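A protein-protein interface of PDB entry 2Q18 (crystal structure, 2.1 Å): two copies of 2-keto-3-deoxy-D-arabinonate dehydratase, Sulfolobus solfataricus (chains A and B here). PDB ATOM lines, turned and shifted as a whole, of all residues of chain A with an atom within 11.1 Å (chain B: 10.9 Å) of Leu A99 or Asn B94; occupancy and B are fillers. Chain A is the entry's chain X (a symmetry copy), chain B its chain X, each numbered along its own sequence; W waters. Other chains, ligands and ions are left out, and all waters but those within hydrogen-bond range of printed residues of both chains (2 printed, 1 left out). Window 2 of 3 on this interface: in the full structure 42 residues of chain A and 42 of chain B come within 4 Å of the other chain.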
ATOM      1  N   VAL A  95      21.357 -12.148  -1.627  1.00  0.00           N
ATOM      2  CA  VAL A  95      22.295 -12.700  -0.644  1.00  0.00           C
ATOM      3  C   VAL A  95      22.691 -14.155  -0.887  1.00  0.00           C
ATOM      4  O   VAL A  95      21.914 -14.942  -1.434  1.00  0.00           O
ATOM      5  CB  VAL A  95      21.762 -12.556   0.806  1.00  0.00           C
ATOM      6  CG1 VAL A  95      22.117 -11.192   1.372  1.00  0.00           C
ATOM      7  CG2 VAL A  95      20.258 -12.792   0.859  1.00  0.00           C
ATOM      8  N   ALA A  96      23.914 -14.493  -0.479  1.00  0.00           N
ATOM      9  CA  ALA A  96      24.390 -15.872  -0.482  1.00  0.00           C
ATOM     10  C   ALA A  96      23.597 -16.684   0.530  1.00  0.00           C
ATOM     11  O   ALA A  96      23.302 -16.207   1.629  1.00  0.00           O
ATOM     12  CB  ALA A  96      25.878 -15.924  -0.158  1.00  0.00           C
ATOM     13  N   LYS A  97      23.242 -17.907   0.154  1.00  0.00           N
ATOM     14  CA  LYS A  97      22.443 -18.759   1.030  1.00  0.00           C
ATOM     15  C   LYS A  97      22.844 -20.232   1.000  1.00  0.00           C
ATOM     16  O   LYS A  97      23.290 -20.750  -0.021  1.00  0.00           O
ATOM     17  CB  LYS A  97      20.941 -18.574   0.764  1.00  0.00           C
ATOM     18  CG  LYS A  97      20.544 -18.490  -0.704  1.00  0.00           C
ATOM     19  CD  LYS A  97      19.567 -17.336  -0.966  1.00  0.00           C
ATOM     20  CE  LYS A  97      18.312 -17.414  -0.103  1.00  0.00           C
ATOM     21  NZ  LYS A  97      17.379 -16.288  -0.388  1.00  0.00           N
ATOM     22  N   ILE A  98      22.695 -20.876   2.153  1.00  0.00           N
ATOM     23  CA  ILE A  98      23.004 -22.287   2.329  1.00  0.00           C
ATOM     24  C   ILE A  98      21.700 -23.022   2.621  1.00  0.00           C
ATOM     25  O   ILE A  98      21.047 -22.761   3.638  1.00  0.00           O
ATOM     26  CB  ILE A  98      24.016 -22.507   3.484  1.00  0.00           C
ATOM     27  CG1 ILE A  98      25.331 -21.771   3.193  1.00  0.00           C
ATOM     28  CG2 ILE A  98      24.263 -24.001   3.716  1.00  0.00           C
ATOM     29  CD1 ILE A  98      26.214 -21.560   4.409  1.00  0.00           C
ATOM     30  N   LEU A  99      21.337 -23.938   1.722  1.00  0.00           N
ATOM     31  CA  LEU A  99      20.032 -24.616   1.742  1.00  0.00           C
ATOM     32  C   LEU A  99      18.873 -23.634   1.954  1.00  0.00           C
ATOM     33  O   LEU A  99      18.054 -23.807   2.861  1.00  0.00           O
ATOM     34  CB  LEU A  99      19.991 -25.748   2.788  1.00  0.00           C
ATOM     35  CG  LEU A  99      20.766 -27.068   2.618  1.00  0.00           C
ATOM     36  CD1 LEU A  99      21.003 -27.444   1.148  1.00  0.00           C
ATOM     37  CD2 LEU A  99      22.082 -27.035   3.379  1.00  0.00           C
ATOM     38  N   GLY A 100      18.830 -22.592   1.123  1.00  0.00           N
ATOM     39  CA  GLY A 100      17.753 -21.598   1.161  1.00  0.00           C
ATOM     40  C   GLY A 100      17.812 -20.576   2.286  1.00  0.00           C
ATOM     41  O   GLY A 100      17.050 -19.604   2.287  1.00  0.00           O
ATOM     42  N   LYS A 101      18.710 -20.790   3.243  1.00  0.00           N
ATOM     43  CA  LYS A 101      18.864 -19.893   4.385  1.00  0.00           C
ATOM     44  C   LYS A 101      20.112 -19.031   4.202  1.00  0.00           C
ATOM     45  O   LYS A 101      21.199 -19.555   3.928  1.00  0.00           O
ATOM     46  CB  LYS A 101      18.957 -20.709   5.676  1.00  0.00           C
ATOM     47  CG  LYS A 101      18.833 -19.908   6.963  1.00  0.00           C
ATOM     48  CD  LYS A 101      18.963 -20.825   8.176  1.00  0.00           C
ATOM     49  CE  LYS A 101      18.745 -20.069   9.477  1.00  0.00           C
ATOM     50  NZ  LYS A 101      18.805 -20.964  10.672  1.00  0.00           N
ATOM     51  N   THR A 102      19.951 -17.716   4.348  1.00  0.00           N
ATOM     52  CA  THR A 102      21.055 -16.772   4.138  1.00  0.00           C
ATOM     53  C   THR A 102      22.189 -17.002   5.138  1.00  0.00           C
ATOM     54  O   THR A 102      21.951 -17.351   6.300  1.00  0.00           O
ATOM     55  CB  THR A 102      20.607 -15.284   4.219  1.00  0.00           C
ATOM     56  OG1 THR A 102      20.512 -14.877   5.589  1.00  0.00           O
ATOM     57  CG2 THR A 102      19.269 -15.065   3.523  1.00  0.00           C
ATOM     58  N   ILE A 103      23.417 -16.797   4.671  1.00  0.00           N
ATOM     59  CA  ILE A 103      24.614 -16.953   5.502  1.00  0.00           C
ATOM     60  C   ILE A 103      24.556 -16.128   6.793  1.00  0.00           C
ATOM     61  O   ILE A 103      25.043 -16.568   7.834  1.00  0.00           O
ATOM     62  CB  ILE A 103      25.913 -16.648   4.708  1.00  0.00           C
ATOM     63  CG1 ILE A 103      25.856 -15.252   4.070  1.00  0.00           C
ATOM     64  CG2 ILE A 103      26.149 -17.729   3.653  1.00  0.00           C
ATOM     65  CD1 ILE A 103      27.178 -14.767   3.492  1.00  0.00           C
ATOM     66  N   TYR A 104      23.940 -14.949   6.720  1.00  0.00           N
ATOM     67  CA  TYR A 104      23.820 -14.048   7.871  1.00  0.00           C
ATOM     68  C   TYR A 104      22.833 -14.580   8.907  1.00  0.00           C
ATOM     69  O   TYR A 104      23.081 -14.501  10.114  1.00  0.00           O
ATOM     70  CB  TYR A 104      23.438 -12.630   7.417  1.00  0.00           C
ATOM     71  CG  TYR A 104      24.440 -12.036   6.452  1.00  0.00           C
ATOM     72  CD1 TYR A 104      25.614 -11.441   6.915  1.00  0.00           C
ATOM     73  CD2 TYR A 104      24.229 -12.095   5.076  1.00  0.00           C
ATOM     74  CE1 TYR A 104      26.547 -10.911   6.034  1.00  0.00           C
ATOM     75  CE2 TYR A 104      25.155 -11.563   4.184  1.00  0.00           C
ATOM     76  CZ  TYR A 104      26.312 -10.973   4.672  1.00  0.00           C
ATOM     77  OH  TYR A 104      27.233 -10.451   3.794  1.00  0.00           O
ATOM     78  N   GLU A 105      21.720 -15.125   8.425  1.00  0.00           N
ATOM     79  CA  GLU A 105      20.732 -15.772   9.285  1.00  0.00           C
ATOM     80  C   GLU A 105      21.335 -17.019   9.947  1.00  0.00           C
ATOM     81  O   GLU A 105      21.087 -17.288  11.125  1.00  0.00           O
ATOM     82  CB  GLU A 105      19.493 -16.143   8.465  1.00  0.00           C
ATOM     83  CG  GLU A 105      18.233 -16.370   9.284  1.00  0.00           C
ATOM     84  CD  GLU A 105      17.091 -16.955   8.460  1.00  0.00           C
ATOM     85  OE1 GLU A 105      17.071 -16.758   7.217  1.00  0.00           O
ATOM     86  OE2 GLU A 105      16.211 -17.614   9.061  1.00  0.00           O
ATOM     87  N   LYS A 106      22.134 -17.760   9.182  1.00  0.00           N
ATOM     88  CA  LYS A 106      22.849 -18.934   9.686  1.00  0.00           C
ATOM     89  C   LYS A 106      23.750 -18.630  10.885  1.00  0.00           C
ATOM     90  O   LYS A 106      23.619 -19.273  11.926  1.00  0.00           O
ATOM     91  CB  LYS A 106      23.657 -19.601   8.574  1.00  0.00           C
ATOM     92  CG  LYS A 106      22.900 -20.678   7.831  1.00  0.00           C
ATOM     93  CD  LYS A 106      23.845 -21.777   7.382  1.00  0.00           C
ATOM     94  CE  LYS A 106      23.124 -23.111   7.292  1.00  0.00           C
ATOM     95  NZ  LYS A 106      24.089 -24.242   7.186  1.00  0.00           N
ATOM     96  N   ASP A 109      21.909 -17.758  14.079  1.00  0.00           N
ATOM     97  CA  ASP A 109      21.327 -18.912  14.774  1.00  0.00           C
ATOM     98  C   ASP A 109      22.357 -19.951  15.240  1.00  0.00           C
ATOM     99  O   ASP A 109      22.010 -20.878  15.976  1.00  0.00           O
ATOM    100  CB  ASP A 109      20.279 -19.593  13.883  1.00  0.00           C
ATOM    101  CG  ASP A 109      19.082 -18.699  13.587  1.00  0.00           C
ATOM    102  OD1 ASP A 109      18.648 -17.942  14.484  1.00  0.00           O
ATOM    103  OD2 ASP A 109      18.568 -18.765  12.453  1.00  0.00           O
ATOM    104  N   ASN B  94      24.815 -27.971   1.587  1.00  0.00           N
ATOM    105  CA  ASN B  94      26.101 -27.843   0.910  1.00  0.00           C
ATOM    106  C   ASN B  94      26.593 -26.390   0.808  1.00  0.00           C
ATOM    107  O   ASN B  94      26.411 -25.604   1.741  1.00  0.00           O
ATOM    108  CB  ASN B  94      26.074 -28.545  -0.462  1.00  0.00           C
ATOM    109  CG  ASN B  94      24.858 -28.164  -1.309  1.00  0.00           C
ATOM    110  OD1 ASN B  94      23.855 -27.652  -0.799  1.00  0.00           O
ATOM    111  ND2 ASN B  94      24.945 -28.425  -2.611  1.00  0.00           N
ATOM    112  N   VAL B  95      27.212 -26.046  -0.319  1.00  0.00           N
ATOM    113  CA  VAL B  95      27.868 -24.748  -0.506  1.00  0.00           C
ATOM    114  C   VAL B  95      26.918 -23.552  -0.540  1.00  0.00           C
ATOM    115  O   VAL B  95      25.763 -23.670  -0.958  1.00  0.00           O
ATOM    116  CB  VAL B  95      28.753 -24.727  -1.780  1.00  0.00           C
ATOM    117  CG1 VAL B  95      30.136 -25.277  -1.478  1.00  0.00           C
ATOM    118  CG2 VAL B  95      28.094 -25.504  -2.913  1.00  0.00           C
ATOM    119  N   ALA B  96      27.422 -22.406  -0.085  1.00  0.00           N
ATOM    120  CA  ALA B  96      26.713 -21.135  -0.199  1.00  0.00           C
ATOM    121  C   ALA B  96      26.596 -20.750  -1.665  1.00  0.00           C
ATOM    122  O   ALA B  96      27.541 -20.922  -2.439  1.00  0.00           O
ATOM    123  CB  ALA B  96      27.439 -20.047   0.582  1.00  0.00           C
ATOM    124  N   LYS B  97      25.432 -20.238  -2.048  1.00  0.00           N
ATOM    125  CA  LYS B  97      25.196 -19.870  -3.440  1.00  0.00           C
ATOM    126  C   LYS B  97      24.381 -18.592  -3.617  1.00  0.00           C
ATOM    127  O   LYS B  97      23.518 -18.269  -2.804  1.00  0.00           O
ATOM    128  CB  LYS B  97      24.589 -21.043  -4.227  1.00  0.00           C
ATOM    129  CG  LYS B  97      23.501 -21.823  -3.501  1.00  0.00           C
ATOM    130  CD  LYS B  97      23.706 -23.338  -3.625  1.00  0.00           C
ATOM    131  CE  LYS B  97      23.789 -23.809  -5.073  1.00  0.00           C
ATOM    132  NZ  LYS B  97      23.975 -25.285  -5.161  1.00  0.00           N
ATOM    133  N   ILE B  98      24.701 -17.867  -4.685  1.00  0.00           N
ATOM    134  CA  ILE B  98      24.033 -16.624  -5.040  1.00  0.00           C
ATOM    135  C   ILE B  98      23.290 -16.848  -6.353  1.00  0.00           C
ATOM    136  O   ILE B  98      23.912 -17.124  -7.386  1.00  0.00           O
ATOM    137  CB  ILE B  98      25.044 -15.457  -5.185  1.00  0.00           C
ATOM    138  CG1 ILE B  98      25.791 -15.228  -3.865  1.00  0.00           C
ATOM    139  CG2 ILE B  98      24.339 -14.178  -5.646  1.00  0.00           C
ATOM    140  CD1 ILE B  98      27.072 -14.425  -4.000  1.00  0.00           C
ATOM    141  N   LEU B  99      21.964 -16.723  -6.299  1.00  0.00           N
ATOM    142  CA  LEU B  99      21.073 -17.073  -7.415  1.00  0.00           C
ATOM    143  C   LEU B  99      21.424 -18.434  -8.030  1.00  0.00           C
ATOM    144  O   LEU B  99      21.634 -18.546  -9.242  1.00  0.00           O
ATOM    145  CB  LEU B  99      21.047 -15.973  -8.494  1.00  0.00           C
ATOM    146  CG  LEU B  99      20.371 -14.607  -8.275  1.00  0.00           C
ATOM    147  CD1 LEU B  99      19.217 -14.660  -7.263  1.00  0.00           C
ATOM    148  CD2 LEU B  99      21.385 -13.548  -7.873  1.00  0.00           C
ATOM    149  N   GLY B 100      21.508 -19.456  -7.179  1.00  0.00           N
ATOM    150  CA  GLY B 100      21.777 -20.829  -7.620  1.00  0.00           C
ATOM    151  C   GLY B 100      23.216 -21.150  -7.997  1.00  0.00           C
ATOM    152  O   GLY B 100      23.561 -22.317  -8.207  1.00  0.00           O
ATOM    153  N   LYS B 101      24.056 -20.122  -8.087  1.00  0.00           N
ATOM    154  CA  LYS B 101      25.460 -20.289  -8.451  1.00  0.00           C
ATOM    155  C   LYS B 101      26.336 -20.156  -7.207  1.00  0.00           C
ATOM    156  O   LYS B 101      26.209 -19.183  -6.454  1.00  0.00           O
ATOM    157  CB  LYS B 101      25.851 -19.246  -9.501  1.00  0.00           C
ATOM    158  CG  LYS B 101      27.192 -19.478 -10.179  1.00  0.00           C
ATOM    159  CD  LYS B 101      27.479 -18.365 -11.184  1.00  0.00           C
ATOM    160  CE  LYS B 101      28.767 -18.620 -11.951  1.00  0.00           C
ATOM    161  NZ  LYS B 101      29.031 -17.574 -12.984  1.00  0.00           N
ATOM    162  N   THR B 102      27.216 -21.134  -6.994  1.00  0.00           N
ATOM    163  CA  THR B 102      28.074 -21.160  -5.804  1.00  0.00           C
ATOM    164  C   THR B 102      29.018 -19.957  -5.766  1.00  0.00           C
ATOM    165  O   THR B 102      29.499 -19.494  -6.807  1.00  0.00           O
ATOM    166  CB  THR B 102      28.917 -22.463  -5.688  1.00  0.00           C
ATOM    167  OG1 THR B 102      30.073 -22.373  -6.528  1.00  0.00           O
ATOM    168  CG2 THR B 102      28.098 -23.692  -6.069  1.00  0.00           C
ATOM    169  N   ILE B 103      29.276 -19.466  -4.557  1.00  0.00           N
ATOM    170  CA  ILE B 103      30.174 -18.329  -4.342  1.00  0.00           C
ATOM    171  C   ILE B 103      31.557 -18.533  -4.971  1.00  0.00           C
ATOM    172  O   ILE B 103      32.160 -17.583  -5.468  1.00  0.00           O
ATOM    173  CB  ILE B 103      30.298 -17.967  -2.837  1.00  0.00           C
ATOM    174  CG1 ILE B 103      30.734 -19.186  -2.010  1.00  0.00           C
ATOM    175  CG2 ILE B 103      28.978 -17.394  -2.324  1.00  0.00           C
ATOM    176  CD1 ILE B 103      31.129 -18.868  -0.575  1.00  0.00           C
ATOM    177  N   TYR B 104      32.037 -19.777  -4.967  1.00  0.00           N
ATOM    178  CA  TYR B 104      33.350 -20.118  -5.522  1.00  0.00           C
ATOM    179  C   TYR B 104      33.358 -20.044  -7.046  1.00  0.00           C
ATOM    180  O   TYR B 104      34.320 -19.558  -7.650  1.00  0.00           O
ATOM    181  CB  TYR B 104      33.808 -21.501  -5.030  1.00  0.00           C
ATOM    182  CG  TYR B 104      33.893 -21.586  -3.522  1.00  0.00           C
ATOM    183  CD1 TYR B 104      35.012 -21.108  -2.840  1.00  0.00           C
ATOM    184  CD2 TYR B 104      32.844 -22.117  -2.776  1.00  0.00           C
ATOM    185  CE1 TYR B 104      35.089 -21.165  -1.455  1.00  0.00           C
ATOM    186  CE2 TYR B 104      32.911 -22.184  -1.387  1.00  0.00           C
ATOM    187  CZ  TYR B 104      34.038 -21.704  -0.735  1.00  0.00           C
ATOM    188  OH  TYR B 104      34.107 -21.763   0.638  1.00  0.00           O
ATOM    189  N   GLU B 105      32.280 -20.526  -7.659  1.00  0.00           N
ATOM    190  CA  GLU B 105      32.095 -20.428  -9.105  1.00  0.00           C
ATOM    191  C   GLU B 105      31.969 -18.958  -9.529  1.00  0.00           C
ATOM    192  O   GLU B 105      32.508 -18.552 -10.561  1.00  0.00           O
ATOM    193  CB  GLU B 105      30.853 -21.219  -9.523  1.00  0.00           C
ATOM    194  CG  GLU B 105      30.809 -21.603 -10.994  1.00  0.00           C
ATOM    195  CD  GLU B 105      29.463 -22.183 -11.412  1.00  0.00           C
ATOM    196  OE1 GLU B 105      28.736 -22.730 -10.542  1.00  0.00           O
ATOM    197  OE2 GLU B 105      29.133 -22.091 -12.618  1.00  0.00           O
ATOM    198  N   TRP B 139      38.369 -31.227  10.196  1.00  0.00           N
ATOM    199  CA  TRP B 139      38.813 -31.388   8.811  1.00  0.00           C
ATOM    200  C   TRP B 139      39.705 -30.229   8.342  1.00  0.00           C
ATOM    201  O   TRP B 139      39.237 -29.267   7.717  1.00  0.00           O
ATOM    202  CB  TRP B 139      37.617 -31.605   7.866  1.00  0.00           C
ATOM    203  CG  TRP B 139      38.009 -31.838   6.436  1.00  0.00           C
ATOM    204  CD1 TRP B 139      39.059 -32.587   5.984  1.00  0.00           C
ATOM    205  CD2 TRP B 139      37.350 -31.325   5.270  1.00  0.00           C
ATOM    206  NE1 TRP B 139      39.099 -32.564   4.610  1.00  0.00           N
ATOM    207  CE2 TRP B 139      38.061 -31.798   4.146  1.00  0.00           C
ATOM    208  CE3 TRP B 139      36.226 -30.512   5.067  1.00  0.00           C
ATOM    209  CZ2 TRP B 139      37.690 -31.483   2.835  1.00  0.00           C
ATOM    210  CZ3 TRP B 139      35.857 -30.198   3.762  1.00  0.00           C
ATOM    211  CH2 TRP B 139      36.589 -30.683   2.664  1.00  0.00           C
ATOM    212  N   ARG B 168      39.028 -26.503   6.670  1.00  0.00           N
ATOM    213  CA  ARG B 168      38.050 -26.602   5.590  1.00  0.00           C
ATOM    214  C   ARG B 168      36.614 -26.847   6.060  1.00  0.00           C
ATOM    215  O   ARG B 168      35.665 -26.418   5.399  1.00  0.00           O
ATOM    216  CB  ARG B 168      38.478 -27.673   4.583  1.00  0.00           C
ATOM    217  CG  ARG B 168      39.727 -27.324   3.770  1.00  0.00           C
ATOM    218  CD  ARG B 168      39.459 -26.250   2.702  1.00  0.00           C
ATOM    219  NE  ARG B 168      38.226 -26.507   1.956  1.00  0.00           N
ATOM    220  CZ  ARG B 168      38.108 -27.391   0.967  1.00  0.00           C
ATOM    221  NH1 ARG B 168      39.153 -28.116   0.579  1.00  0.00           N
ATOM    222  NH2 ARG B 168      36.939 -27.554   0.364  1.00  0.00           N
ATOM    223  N   ASP B 169      36.458 -27.518   7.199  1.00  0.00           N
ATOM    224  CA  ASP B 169      35.127 -27.787   7.747  1.00  0.00           C
ATOM    225  C   ASP B 169      34.437 -26.515   8.230  1.00  0.00           C
ATOM    226  O   ASP B 169      33.236 -26.344   8.018  1.00  0.00           O
ATOM    227  CB  ASP B 169      35.169 -28.850   8.858  1.00  0.00           C
ATOM    228  CG  ASP B 169      36.107 -28.488  10.000  1.00  0.00           C
ATOM    229  OD1 ASP B 169      37.167 -27.869   9.746  1.00  0.00           O
ATOM    230  OD2 ASP B 169      35.784 -28.836  11.158  1.00  0.00           O
ATOM    231  N   LEU B 170      35.200 -25.624   8.867  1.00  0.00           N
ATOM    232  CA  LEU B 170      34.658 -24.353   9.346  1.00  0.00           C
ATOM    233  C   LEU B 170      34.240 -23.460   8.176  1.00  0.00           C
ATOM    234  O   LEU B 170      33.196 -22.809   8.227  1.00  0.00           O
ATOM    235  CB  LEU B 170      35.650 -23.634  10.273  1.00  0.00           C
ATOM    236  CG  LEU B 170      36.135 -24.364  11.536  1.00  0.00           C
ATOM    237  CD1 LEU B 170      36.950 -23.432  12.432  1.00  0.00           C
ATOM    238  CD2 LEU B 170      34.984 -24.977  12.325  1.00  0.00           C
ATOM    239  N   GLU B 171      35.052 -23.459   7.121  1.00  0.00           N
ATOM    240  CA  GLU B 171      34.755 -22.735   5.891  1.00  0.00           C
ATOM    241  C   GLU B 171      33.477 -23.243   5.203  1.00  0.00           C
ATOM    242  O   GLU B 171      32.649 -22.443   4.751  1.00  0.00           O
ATOM    243  CB  GLU B 171      35.944 -22.828   4.932  1.00  0.00           C
ATOM    244  CG  GLU B 171      35.648 -22.329   3.528  1.00  0.00           C
ATOM    245  CD  GLU B 171      36.816 -22.476   2.572  1.00  0.00           C
ATOM    246  OE1 GLU B 171      37.817 -23.147   2.918  1.00  0.00           O
ATOM    247  OE2 GLU B 171      36.725 -21.914   1.460  1.00  0.00           O
ATOM    248  N   ALA B 172      33.335 -24.568   5.121  1.00  0.00           N
ATOM    249  CA  ALA B 172      32.181 -25.205   4.480  1.00  0.00           C
ATOM    250  C   ALA B 172      30.895 -24.913   5.241  1.00  0.00           C
ATOM    251  O   ALA B 172      29.821 -24.795   4.648  1.00  0.00           O
ATOM    252  CB  ALA B 172      32.400 -26.710   4.361  1.00  0.00           C
ATOM    253  N   GLU B 173      31.025 -24.797   6.557  1.00  0.00           N
ATOM    254  CA  GLU B 173      29.930 -24.475   7.462  1.00  0.00           C
ATOM    255  C   GLU B 173      29.293 -23.113   7.126  1.00  0.00           C
ATOM    256  O   GLU B 173      28.067 -22.967   7.142  1.00  0.00           O
ATOM    257  CB  GLU B 173      30.492 -24.444   8.878  1.00  0.00           C
ATOM    258  CG  GLU B 173      29.669 -25.116   9.934  1.00  0.00           C
ATOM    259  CD  GLU B 173      30.516 -25.490  11.137  1.00  0.00           C
ATOM    260  OE1 GLU B 173      31.224 -26.524  11.073  1.00  0.00           O
ATOM    261  OE2 GLU B 173      30.481 -24.750  12.144  1.00  0.00           O
ATOM    262  N   ASN B 174      30.140 -22.127   6.825  1.00  0.00           N
ATOM    263  CA  ASN B 174      29.712 -20.767   6.479  1.00  0.00           C
ATOM    264  C   ASN B 174      30.918 -19.989   5.957  1.00  0.00           C
ATOM    265  O   ASN B 174      31.965 -19.984   6.605  1.00  0.00           O
ATOM    266  CB  ASN B 174      29.123 -20.059   7.707  1.00  0.00           C
ATOM    267  CG  ASN B 174      28.242 -18.873   7.348  1.00  0.00           C
ATOM    268  OD1 ASN B 174      28.619 -18.017   6.550  1.00  0.00           O
ATOM    269  ND2 ASN B 174      27.059 -18.812   7.955  1.00  0.00           N
ATOM    270  N   PRO B 175      30.785 -19.337   4.780  1.00  0.00           N
ATOM    271  CA  PRO B 175      31.875 -18.505   4.242  1.00  0.00           C
ATOM    272  C   PRO B 175      32.288 -17.365   5.177  1.00  0.00           C
ATOM    273  O   PRO B 175      33.400 -16.845   5.060  1.00  0.00           O
ATOM    274  CB  PRO B 175      31.287 -17.939   2.945  1.00  0.00           C
ATOM    275  CG  PRO B 175      29.802 -18.111   3.070  1.00  0.00           C
ATOM    276  CD  PRO B 175      29.614 -19.351   3.882  1.00  0.00           C
ATOM    277  N   LEU B 176      31.402 -16.998   6.100  1.00  0.00           N
ATOM    278  CA  LEU B 176      31.686 -15.968   7.095  1.00  0.00           C
ATOM    279  C   LEU B 176      32.632 -16.456   8.195  1.00  0.00           C
ATOM    280  O   LEU B 176      33.106 -15.656   9.010  1.00  0.00           O
ATOM    281  CB  LEU B 176      30.384 -15.426   7.703  1.00  0.00           C
ATOM    282  CG  LEU B 176      29.412 -14.707   6.751  1.00  0.00           C
ATOM    283  CD1 LEU B 176      28.168 -14.262   7.501  1.00  0.00           C
ATOM    284  CD2 LEU B 176      30.073 -13.514   6.051  1.00  0.00           C
ATOM    285  N   ARG B 262      37.843 -35.458   1.688  1.00  0.00           N
ATOM    286  CA  ARG B 262      37.238 -35.193   2.992  1.00  0.00           C
ATOM    287  C   ARG B 262      37.732 -36.134   4.093  1.00  0.00           C
ATOM    288  O   ARG B 262      37.606 -35.826   5.281  1.00  0.00           O
ATOM    289  CB  ARG B 262      35.709 -35.246   2.891  1.00  0.00           C
ATOM    290  CG  ARG B 262      34.986 -34.464   3.987  1.00  0.00           C
ATOM    291  CD  ARG B 262      33.519 -34.237   3.639  1.00  0.00           C
ATOM    292  NE  ARG B 262      33.358 -33.421   2.436  1.00  0.00           N
ATOM    293  CZ  ARG B 262      32.191 -33.151   1.854  1.00  0.00           C
ATOM    294  NH1 ARG B 262      32.158 -32.398   0.761  1.00  0.00           N
ATOM    295  NH2 ARG B 262      31.056 -33.629   2.358  1.00  0.00           N
HETATM  296  O   HOH W   1      20.729 -15.838  -3.805  1.00  0.00           O
HETATM  297  O   HOH W   2      23.151 -24.552  -0.483  1.00  0.00           O
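Printed residues of chain B that touch a printed residue of chain A: Asn B94, Val B95, Ala B96, Lys B97, Ile B98, Glu B173, Asn B174, Pro B175 and Leu B176.
Hydrophobic or aromatic side chains of chain B that line the printed part of chain A: Ala B96, Ile B98, Pro B175 and Leu B176.
Printed residues of chain A that touch a printed residue of chain B: Val A95, Ala A96, Lys A97, Ile A98, Leu A99, Ile A103, Tyr A104 and Lys A106.
Among the printed residues, no Asp or Glu carboxylate lies within 4 Å of a Lys or Arg side-chain nitrogen of the other chain.
O of Ala B96 is in hydrogen-bond range of N of Ile B103 (3.1 Å).
The side-chain amide oxygen of Asn B174 sits at hydrogen-bond distance from the backbone NH of Leu B176, at 3.0 Å.
The backbone NH of Ile A103 lies within hydrogen-bond range of the backbone carbonyl oxygen of Ala A96, at 3.1 Å.
Asn B94 touches just these residues of chain A: Ile A98 (3.3 Å) and Leu A99 (3.4 Å).
Printed residues of chain B within 4 Å of Ile A98: Asn B94, Ala B96 and Glu B173.
Gly A100 touches none of the printed residues of chain B.
Printed residues of chain A within 4 Å of Val B95: Lys A97 (3.9 Å).
Ala B96 touches just these residues of chain A: Lys A97 and Ile A98.
Of the printed residues of chain B, Tyr A104 touches Leu B176.
Of the printed residues of chain B, Val A95 touches Lys B97 (3.9 Å).
Printed residues of chain A within 4 Å of Glu B173: Ile A98 (3.6 Å).
The nearest printed residue of chain A that does not touch Glu B173 is Lys A106 (4.2 Å).
Val A95 touches Lys B97, and with the chains exchanged Lys A97 touches Val B95.
Ala A96 touches Lys B97, and with the chains exchanged Lys A97 touches Ala B96.
Ala A96 touches Ile B98, and with the chains exchanged Ile A98 touches Ala B96.
Lys B97 touches its own counterpart, Lys A97.
11 positions are printed for both chains.
Of the 15 pairs that touch across the chains among the printed residues, 7 have their exchanged pair printed and touching as well.
Among the printed residues, merely in contact across the chains: Ile A98 with Asn B94 (3.3 Å), Leu A99 with Asn B94 (3.4 Å), Lys A97 with Ala B96 (3.4 Å), Ala A96 with Lys B97 (3.4 Å), Lys A106 with Asn B174 (3.5 Å), Ile A98 with Glu B173 (3.6 Å), Ile A98 with Ala B96 (3.7 Å), Ala A96 with Ile B98 (3.7 Å), Ile A103 with Pro B175 (3.7 Å), Tyr A104 with Leu B176 (3.9 Å), Ile A103 with Leu B176 (3.9 Å), Val A95 with Lys B97 (3.9 Å) and Lys A97 with Val B95 (3.9 Å).
N of Lys B97 sits at hydrogen-bond distance from O of Lys A97, at 3.0 Å.
The side-chain amide nitrogen (ND2) of Asn B174 sits at hydrogen-bond distance from the backbone carbonyl oxygen (O) of Ile A103 (3.0 Å).
Water W2 lies within hydrogen-bond range of O of Val B95 (2.8 Å), N of Leu A99 (2.9 Å) and OD1 of Asn B94 (3.2 Å).
Water W1 bridges O of Val A95 (2.8 Å) and N of Leu B99 (2.9 Å).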
